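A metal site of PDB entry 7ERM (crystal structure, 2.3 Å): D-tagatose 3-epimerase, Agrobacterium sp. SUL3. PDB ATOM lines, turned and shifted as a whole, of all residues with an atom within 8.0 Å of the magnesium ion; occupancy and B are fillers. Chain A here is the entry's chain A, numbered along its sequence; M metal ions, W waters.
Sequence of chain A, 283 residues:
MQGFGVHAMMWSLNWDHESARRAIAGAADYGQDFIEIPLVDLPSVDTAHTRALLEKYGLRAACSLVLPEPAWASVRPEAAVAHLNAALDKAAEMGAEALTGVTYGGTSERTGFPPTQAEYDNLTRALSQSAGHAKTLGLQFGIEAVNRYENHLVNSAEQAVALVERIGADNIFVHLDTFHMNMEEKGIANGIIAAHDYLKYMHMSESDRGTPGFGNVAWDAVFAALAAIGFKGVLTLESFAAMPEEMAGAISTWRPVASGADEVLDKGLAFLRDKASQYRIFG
The magnesium ion is bound by OD2 of Asp 177 (2.0 Å), OE2 of Glu 144 (2.0 Å), ND1 of His 203 (2.0 Å), OE1 of Glu 238 (2.2 Å) and water W1 (2.4 Å). The magnesium ion has five donor atoms within binding distance.
The side-chain carboxylate (OD1) of Asp 177 lies within salt-bridge range of the guanidinium group (NH1) of Arg 209 (3.3 Å). The backbone NH of Phe 179 lies within hydrogen-bond range of the side-chain carboxylate of Asp 177 (3.0 Å). O of Leu 176 sits at hydrogen-bond distance from N of His 203 (2.7 Å). A ring nitrogen (NE2) of His 203 sits at hydrogen-bond distance from the side-chain carboxylate of Glu 36, 2.9 Å away. The backbone carbonyl oxygen (O) of His 203 sits at hydrogen-bond distance from the backbone NH (N) of Thr 178 (3.0 Å). The side-chain carboxylate of Glu 238 lies close to the guanidinium group of Arg 209 (3.2 Å). The side-chain hydroxyl (OG) of Ser 205 lies within hydrogen-bond range of the backbone carbonyl oxygen (O) of Glu 238 (2.7 Å). N of Glu 238 is in hydrogen-bond range of O of Met 204 (3.3 Å).
Four residues have an atom within 4 Å of the magnesium ion: Glu 144, Asp 177, His 203 and Glu 238. Along chain A the residues within 4 Å of the magnesium ion span positions 144 to 238.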
ATOM      1  N   HIS A   7      19.177  30.318 -13.664  1.00  0.00           N
ATOM      2  CA  HIS A   7      18.408  31.054 -12.674  1.00  0.00           C
ATOM      3  C   HIS A   7      17.591  32.159 -13.331  1.00  0.00           C
ATOM      4  O   HIS A   7      18.095  32.893 -14.179  1.00  0.00           O
ATOM      5  CB  HIS A   7      19.346  31.650 -11.630  1.00  0.00           C
ATOM      6  CG  HIS A   7      18.672  32.047 -10.368  1.00  0.00           C
ATOM      7  ND1 HIS A   7      17.740  33.072 -10.321  1.00  0.00           N
ATOM      8  CD2 HIS A   7      18.770  31.570  -9.106  1.00  0.00           C
ATOM      9  CE1 HIS A   7      17.312  33.215  -9.082  1.00  0.00           C
ATOM     10  NE2 HIS A   7      17.921  32.320  -8.317  1.00  0.00           N
ATOM     11  N   MET A   9      16.853  34.998 -12.413  1.00  0.00           N
ATOM     12  CA  MET A   9      17.400  36.346 -12.291  1.00  0.00           C
ATOM     13  C   MET A   9      18.019  36.862 -13.593  1.00  0.00           C
ATOM     14  O   MET A   9      18.182  38.078 -13.749  1.00  0.00           O
ATOM     15  CB  MET A   9      18.450  36.392 -11.173  1.00  0.00           C
ATOM     16  CG  MET A   9      19.759  35.650 -11.474  1.00  0.00           C
ATOM     17  SD  MET A   9      20.921  35.737 -10.098  1.00  0.00           S
ATOM     18  CE  MET A   9      19.941  35.173  -8.699  1.00  0.00           C
ATOM     19  N   GLU A  36      15.455  27.941 -12.549  1.00  0.00           N
ATOM     20  CA  GLU A  36      15.338  28.072 -11.106  1.00  0.00           C
ATOM     21  C   GLU A  36      14.528  29.319 -10.795  1.00  0.00           C
ATOM     22  O   GLU A  36      14.904  30.424 -11.178  1.00  0.00           O
ATOM     23  CB  GLU A  36      16.712  28.152 -10.453  1.00  0.00           C
ATOM     24  CG  GLU A  36      16.667  28.146  -8.952  1.00  0.00           C
ATOM     25  CD  GLU A  36      18.038  28.305  -8.315  1.00  0.00           C
ATOM     26  OE1 GLU A  36      18.977  27.633  -8.774  1.00  0.00           O
ATOM     27  OE2 GLU A  36      18.174  29.094  -7.358  1.00  0.00           O
ATOM     28  N   SER A  64      13.897  28.342  -5.336  1.00  0.00           N
ATOM     29  CA  SER A  64      14.904  28.671  -4.330  1.00  0.00           C
ATOM     30  C   SER A  64      14.480  29.909  -3.529  1.00  0.00           C
ATOM     31  O   SER A  64      13.689  30.729  -3.992  1.00  0.00           O
ATOM     32  CB  SER A  64      16.286  28.891  -4.961  1.00  0.00           C
ATOM     33  OG  SER A  64      16.304  29.979  -5.875  1.00  0.00           O
ATOM     34  N   GLY A 101      18.549  26.651  -2.023  1.00  0.00           N
ATOM     35  CA  GLY A 101      19.004  27.984  -1.672  1.00  0.00           C
ATOM     36  C   GLY A 101      19.379  28.089  -0.201  1.00  0.00           C
ATOM     37  O   GLY A 101      19.720  27.103   0.459  1.00  0.00           O
ATOM     38  N   VAL A 102      19.337  29.324   0.302  1.00  0.00           N
ATOM     39  CA  VAL A 102      19.659  29.586   1.701  1.00  0.00           C
ATOM     40  C   VAL A 102      18.426  29.280   2.540  1.00  0.00           C
ATOM     41  O   VAL A 102      17.693  30.192   2.967  1.00  0.00           O
ATOM     42  CB  VAL A 102      20.178  31.022   1.895  1.00  0.00           C
ATOM     43  CG1 VAL A 102      20.681  31.259   3.321  1.00  0.00           C
ATOM     44  CG2 VAL A 102      21.293  31.269   0.922  1.00  0.00           C
ATOM     45  N   GLU A 144      22.212  25.269   0.454  1.00  0.00           N
ATOM     46  CA  GLU A 144      23.276  25.931  -0.311  1.00  0.00           C
ATOM     47  C   GLU A 144      24.251  26.590   0.669  1.00  0.00           C
ATOM     48  O   GLU A 144      23.884  27.516   1.382  1.00  0.00           O
ATOM     49  CB  GLU A 144      22.728  26.975  -1.283  1.00  0.00           C
ATOM     50  CG  GLU A 144      23.833  27.653  -2.172  1.00  0.00           C
ATOM     51  CD  GLU A 144      23.326  28.768  -3.128  1.00  0.00           C
ATOM     52  OE1 GLU A 144      22.095  29.002  -3.165  1.00  0.00           O
ATOM     53  OE2 GLU A 144      24.156  29.402  -3.846  1.00  0.00           O
ATOM     54  N   ALA A 145      25.499  26.111   0.677  1.00  0.00           N
ATOM     55  CA  ALA A 145      26.568  26.784   1.414  1.00  0.00           C
ATOM     56  C   ALA A 145      26.907  28.125   0.752  1.00  0.00           C
ATOM     57  O   ALA A 145      27.045  28.215  -0.470  1.00  0.00           O
ATOM     58  CB  ALA A 145      27.806  25.898   1.469  1.00  0.00           C
ATOM     59  N   VAL A 146      27.062  29.172   1.571  1.00  0.00           N
ATOM     60  CA  VAL A 146      27.444  30.501   1.108  1.00  0.00           C
ATOM     61  C   VAL A 146      28.628  30.997   1.939  1.00  0.00           C
ATOM     62  O   VAL A 146      28.960  30.440   2.982  1.00  0.00           O
ATOM     63  CB  VAL A 146      26.273  31.505   1.157  1.00  0.00           C
ATOM     64  CG1 VAL A 146      25.154  31.074   0.195  1.00  0.00           C
ATOM     65  CG2 VAL A 146      25.729  31.649   2.567  1.00  0.00           C
ATOM     66  N   GLU A 150      28.006  36.496   4.126  1.00  0.00           N
ATOM     67  CA  GLU A 150      26.564  36.407   3.998  1.00  0.00           C
ATOM     68  C   GLU A 150      25.944  35.656   5.150  1.00  0.00           C
ATOM     69  O   GLU A 150      24.825  35.959   5.572  1.00  0.00           O
ATOM     70  CB  GLU A 150      26.204  35.723   2.677  1.00  0.00           C
ATOM     71  CG  GLU A 150      26.774  36.440   1.453  1.00  0.00           C
ATOM     72  CD  GLU A 150      26.007  36.153   0.144  1.00  0.00           C
ATOM     73  OE1 GLU A 150      26.364  36.744  -0.909  1.00  0.00           O
ATOM     74  OE2 GLU A 150      25.042  35.347   0.161  1.00  0.00           O
ATOM     75  N   HIS A 175      23.964  21.671  -1.922  1.00  0.00           N
ATOM     76  CA  HIS A 175      23.965  22.567  -3.074  1.00  0.00           C
ATOM     77  C   HIS A 175      25.187  23.479  -2.932  1.00  0.00           C
ATOM     78  O   HIS A 175      25.337  24.152  -1.916  1.00  0.00           O
ATOM     79  CB  HIS A 175      22.616  23.339  -3.097  1.00  0.00           C
ATOM     80  CG  HIS A 175      22.543  24.465  -4.085  1.00  0.00           C
ATOM     81  ND1 HIS A 175      21.393  25.215  -4.260  1.00  0.00           N
ATOM     82  CD2 HIS A 175      23.464  24.982  -4.939  1.00  0.00           C
ATOM     83  CE1 HIS A 175      21.611  26.136  -5.173  1.00  0.00           C
ATOM     84  NE2 HIS A 175      22.862  26.029  -5.588  1.00  0.00           N
ATOM     85  N   LEU A 176      26.075  23.490  -3.944  1.00  0.00           N
ATOM     86  CA  LEU A 176      27.281  24.302  -3.904  1.00  0.00           C
ATOM     87  C   LEU A 176      27.252  25.409  -4.968  1.00  0.00           C
ATOM     88  O   LEU A 176      26.565  25.297  -5.995  1.00  0.00           O
ATOM     89  CB  LEU A 176      28.547  23.437  -4.048  1.00  0.00           C
ATOM     90  CG  LEU A 176      28.694  22.392  -2.922  1.00  0.00           C
ATOM     91  CD1 LEU A 176      29.857  21.426  -3.100  1.00  0.00           C
ATOM     92  CD2 LEU A 176      28.798  23.057  -1.588  1.00  0.00           C
ATOM     93  N   ASP A 177      28.001  26.482  -4.695  1.00  0.00           N
ATOM     94  CA  ASP A 177      27.987  27.692  -5.512  1.00  0.00           C
ATOM     95  C   ASP A 177      29.445  28.077  -5.738  1.00  0.00           C
ATOM     96  O   ASP A 177      30.157  28.393  -4.777  1.00  0.00           O
ATOM     97  CB  ASP A 177      27.191  28.804  -4.807  1.00  0.00           C
ATOM     98  CG  ASP A 177      27.086  30.107  -5.631  1.00  0.00           C
ATOM     99  OD1 ASP A 177      28.072  30.489  -6.290  1.00  0.00           O
ATOM    100  OD2 ASP A 177      25.996  30.745  -5.586  1.00  0.00           O
ATOM    101  N   THR A 178      29.910  28.030  -7.008  1.00  0.00           N
ATOM    102  CA  THR A 178      31.340  28.193  -7.260  1.00  0.00           C
ATOM    103  C   THR A 178      31.855  29.577  -6.879  1.00  0.00           C
ATOM    104  O   THR A 178      33.026  29.706  -6.529  1.00  0.00           O
ATOM    105  CB  THR A 178      31.698  27.879  -8.728  1.00  0.00           C
ATOM    106  OG1 THR A 178      30.921  28.688  -9.629  1.00  0.00           O
ATOM    107  CG2 THR A 178      31.493  26.413  -9.006  1.00  0.00           C
ATOM    108  N   PHE A 179      31.022  30.606  -6.958  1.00  0.00           N
ATOM    109  CA  PHE A 179      31.402  31.919  -6.424  1.00  0.00           C
ATOM    110  C   PHE A 179      31.742  31.835  -4.942  1.00  0.00           C
ATOM    111  O   PHE A 179      32.711  32.446  -4.480  1.00  0.00           O
ATOM    112  CB  PHE A 179      30.276  32.934  -6.657  1.00  0.00           C
ATOM    113  CG  PHE A 179      30.461  34.243  -5.925  1.00  0.00           C
ATOM    114  CD1 PHE A 179      31.154  35.287  -6.510  1.00  0.00           C
ATOM    115  CD2 PHE A 179      29.899  34.445  -4.662  1.00  0.00           C
ATOM    116  CE1 PHE A 179      31.309  36.500  -5.847  1.00  0.00           C
ATOM    117  CE2 PHE A 179      30.068  35.647  -3.995  1.00  0.00           C
ATOM    118  CZ  PHE A 179      30.769  36.681  -4.585  1.00  0.00           C
ATOM    119  N   HIS A 180      30.936  31.095  -4.172  1.00  0.00           N
ATOM    120  CA  HIS A 180      31.162  30.961  -2.730  1.00  0.00           C
ATOM    121  C   HIS A 180      32.293  29.973  -2.419  1.00  0.00           C
ATOM    122  O   HIS A 180      33.078  30.231  -1.502  1.00  0.00           O
ATOM    123  CB  HIS A 180      29.887  30.512  -2.045  1.00  0.00           C
ATOM    124  CG  HIS A 180      28.795  31.537  -2.061  1.00  0.00           C
ATOM    125  ND1 HIS A 180      28.995  32.826  -1.636  1.00  0.00           N
ATOM    126  CD2 HIS A 180      27.499  31.457  -2.465  1.00  0.00           C
ATOM    127  CE1 HIS A 180      27.861  33.501  -1.756  1.00  0.00           C
ATOM    128  NE2 HIS A 180      26.941  32.684  -2.259  1.00  0.00           N
ATOM    129  N   TYR A 201      23.138  19.604  -6.874  1.00  0.00           N
ATOM    130  CA  TYR A 201      22.810  20.897  -7.468  1.00  0.00           C
ATOM    131  C   TYR A 201      24.032  21.796  -7.361  1.00  0.00           C
ATOM    132  O   TYR A 201      24.637  21.874  -6.290  1.00  0.00           O
ATOM    133  CB  TYR A 201      21.624  21.524  -6.737  1.00  0.00           C
ATOM    134  CG  TYR A 201      20.836  22.500  -7.571  1.00  0.00           C
ATOM    135  CD1 TYR A 201      21.188  23.839  -7.619  1.00  0.00           C
ATOM    136  CD2 TYR A 201      19.714  22.080  -8.316  1.00  0.00           C
ATOM    137  CE1 TYR A 201      20.454  24.740  -8.375  1.00  0.00           C
ATOM    138  CE2 TYR A 201      18.985  22.971  -9.063  1.00  0.00           C
ATOM    139  CZ  TYR A 201      19.362  24.301  -9.091  1.00  0.00           C
ATOM    140  OH  TYR A 201      18.653  25.223  -9.829  1.00  0.00           O
ATOM    141  N   MET A 202      24.383  22.484  -8.440  1.00  0.00           N
ATOM    142  CA  MET A 202      25.435  23.489  -8.444  1.00  0.00           C
ATOM    143  C   MET A 202      24.903  24.828  -8.956  1.00  0.00           C
ATOM    144  O   MET A 202      24.124  24.878  -9.910  1.00  0.00           O
ATOM    145  CB  MET A 202      26.620  23.076  -9.357  1.00  0.00           C
ATOM    146  CG  MET A 202      27.352  21.843  -8.923  1.00  0.00           C
ATOM    147  SD  MET A 202      28.437  22.175  -7.537  1.00  0.00           S
ATOM    148  CE  MET A 202      29.486  23.438  -8.216  1.00  0.00           C
ATOM    149  N   HIS A 203      25.361  25.905  -8.338  1.00  0.00           N
ATOM    150  CA  HIS A 203      25.340  27.222  -8.979  1.00  0.00           C
ATOM    151  C   HIS A 203      26.684  27.417  -9.667  1.00  0.00           C
ATOM    152  O   HIS A 203      27.714  27.542  -8.997  1.00  0.00           O
ATOM    153  CB  HIS A 203      25.082  28.332  -7.978  1.00  0.00           C
ATOM    154  CG  HIS A 203      23.640  28.546  -7.673  1.00  0.00           C
ATOM    155  ND1 HIS A 203      23.212  29.373  -6.650  1.00  0.00           N
ATOM    156  CD2 HIS A 203      22.527  28.050  -8.263  1.00  0.00           C
ATOM    157  CE1 HIS A 203      21.890  29.365  -6.623  1.00  0.00           C
ATOM    158  NE2 HIS A 203      21.447  28.576  -7.594  1.00  0.00           N
ATOM    159  N   MET A 204      26.651  27.483 -11.002  1.00  0.00           N
ATOM    160  CA  MET A 204      27.857  27.694 -11.794  1.00  0.00           C
ATOM    161  C   MET A 204      27.940  29.187 -12.024  1.00  0.00           C
ATOM    162  O   MET A 204      27.328  29.736 -12.943  1.00  0.00           O
ATOM    163  CB  MET A 204      27.814  26.889 -13.085  1.00  0.00           C
ATOM    164  CG  MET A 204      27.645  25.370 -12.856  1.00  0.00           C
ATOM    165  SD  MET A 204      28.982  24.562 -11.938  1.00  0.00           S
ATOM    166  CE  MET A 204      29.938  23.932 -13.321  1.00  0.00           C
ATOM    167  N   SER A 205      28.708  29.853 -11.160  1.00  0.00           N
ATOM    168  CA  SER A 205      28.780  31.303 -11.106  1.00  0.00           C
ATOM    169  C   SER A 205      30.236  31.729 -11.118  1.00  0.00           C
ATOM    170  O   SER A 205      31.062  31.129 -10.431  1.00  0.00           O
ATOM    171  CB  SER A 205      28.066  31.831  -9.851  1.00  0.00           C
ATOM    172  OG  SER A 205      27.780  33.219  -9.952  1.00  0.00           O
ATOM    173  N   ARG A 209      30.446  37.152 -10.128  1.00  0.00           N
ATOM    174  CA  ARG A 209      29.038  37.045 -10.552  1.00  0.00           C
ATOM    175  C   ARG A 209      28.830  37.530 -11.982  1.00  0.00           C
ATOM    176  O   ARG A 209      27.701  37.859 -12.356  1.00  0.00           O
ATOM    177  CB  ARG A 209      28.090  37.804  -9.603  1.00  0.00           C
ATOM    178  CG  ARG A 209      28.172  37.399  -8.120  1.00  0.00           C
ATOM    179  CD  ARG A 209      27.819  35.931  -7.942  1.00  0.00           C
ATOM    180  NE  ARG A 209      27.246  35.634  -6.638  1.00  0.00           N
ATOM    181  CZ  ARG A 209      26.809  34.418  -6.278  1.00  0.00           C
ATOM    182  NH1 ARG A 209      26.858  33.410  -7.137  1.00  0.00           N
ATOM    183  NH2 ARG A 209      26.308  34.221  -5.064  1.00  0.00           N
ATOM    184  N   THR A 236      23.258  24.853 -12.741  1.00  0.00           N
ATOM    185  CA  THR A 236      22.501  26.064 -12.989  1.00  0.00           C
ATOM    186  C   THR A 236      23.434  27.275 -12.990  1.00  0.00           C
ATOM    187  O   THR A 236      24.198  27.487 -12.044  1.00  0.00           O
ATOM    188  CB  THR A 236      21.400  26.235 -11.947  1.00  0.00           C
ATOM    189  OG1 THR A 236      20.426  25.198 -12.147  1.00  0.00           O
ATOM    190  CG2 THR A 236      20.732  27.583 -12.095  1.00  0.00           C
ATOM    191  N   LEU A 237      23.362  28.052 -14.051  1.00  0.00           N
ATOM    192  CA  LEU A 237      24.125  29.292 -14.133  1.00  0.00           C
ATOM    193  C   LEU A 237      23.475  30.364 -13.269  1.00  0.00           C
ATOM    194  O   LEU A 237      22.255  30.531 -13.261  1.00  0.00           O
ATOM    195  CB  LEU A 237      24.173  29.777 -15.575  1.00  0.00           C
ATOM    196  CG  LEU A 237      25.021  31.008 -15.820  1.00  0.00           C
ATOM    197  CD1 LEU A 237      25.984  30.742 -16.970  1.00  0.00           C
ATOM    198  CD2 LEU A 237      24.116  32.179 -16.125  1.00  0.00           C
ATOM    199  N   GLU A 238      24.308  31.095 -12.537  1.00  0.00           N
ATOM    200  CA  GLU A 238      23.865  32.242 -11.753  1.00  0.00           C
ATOM    201  C   GLU A 238      24.797  33.403 -12.061  1.00  0.00           C
ATOM    202  O   GLU A 238      26.012  33.259 -11.935  1.00  0.00           O
ATOM    203  CB  GLU A 238      23.852  31.891 -10.260  1.00  0.00           C
ATOM    204  CG  GLU A 238      23.878  33.050  -9.269  1.00  0.00           C
ATOM    205  CD  GLU A 238      23.456  32.626  -7.862  1.00  0.00           C
ATOM    206  OE1 GLU A 238      24.132  31.788  -7.205  1.00  0.00           O
ATOM    207  OE2 GLU A 238      22.396  33.109  -7.431  1.00  0.00           O
ATOM    208  N   PHE A 240      24.743  38.073 -12.029  1.00  0.00           N
ATOM    209  CA  PHE A 240      24.017  39.290 -11.676  1.00  0.00           C
ATOM    210  C   PHE A 240      23.900  40.289 -12.842  1.00  0.00           C
ATOM    211  O   PHE A 240      23.581  41.459 -12.608  1.00  0.00           O
ATOM    212  CB  PHE A 240      24.679  39.991 -10.482  1.00  0.00           C
ATOM    213  CG  PHE A 240      24.504  39.267  -9.181  1.00  0.00           C
ATOM    214  CD1 PHE A 240      23.892  38.028  -9.125  1.00  0.00           C
ATOM    215  CD2 PHE A 240      24.995  39.821  -8.009  1.00  0.00           C
ATOM    216  CE1 PHE A 240      23.751  37.355  -7.909  1.00  0.00           C
ATOM    217  CE2 PHE A 240      24.855  39.158  -6.793  1.00  0.00           C
ATOM    218  CZ  PHE A 240      24.231  37.919  -6.754  1.00  0.00           C
HETATM  219 MG    MG M   1      24.049  30.627  -5.382  1.00  0.00          MG
HETATM  220  O   HOH W   1      22.374  31.885  -4.136  1.00  0.00           O
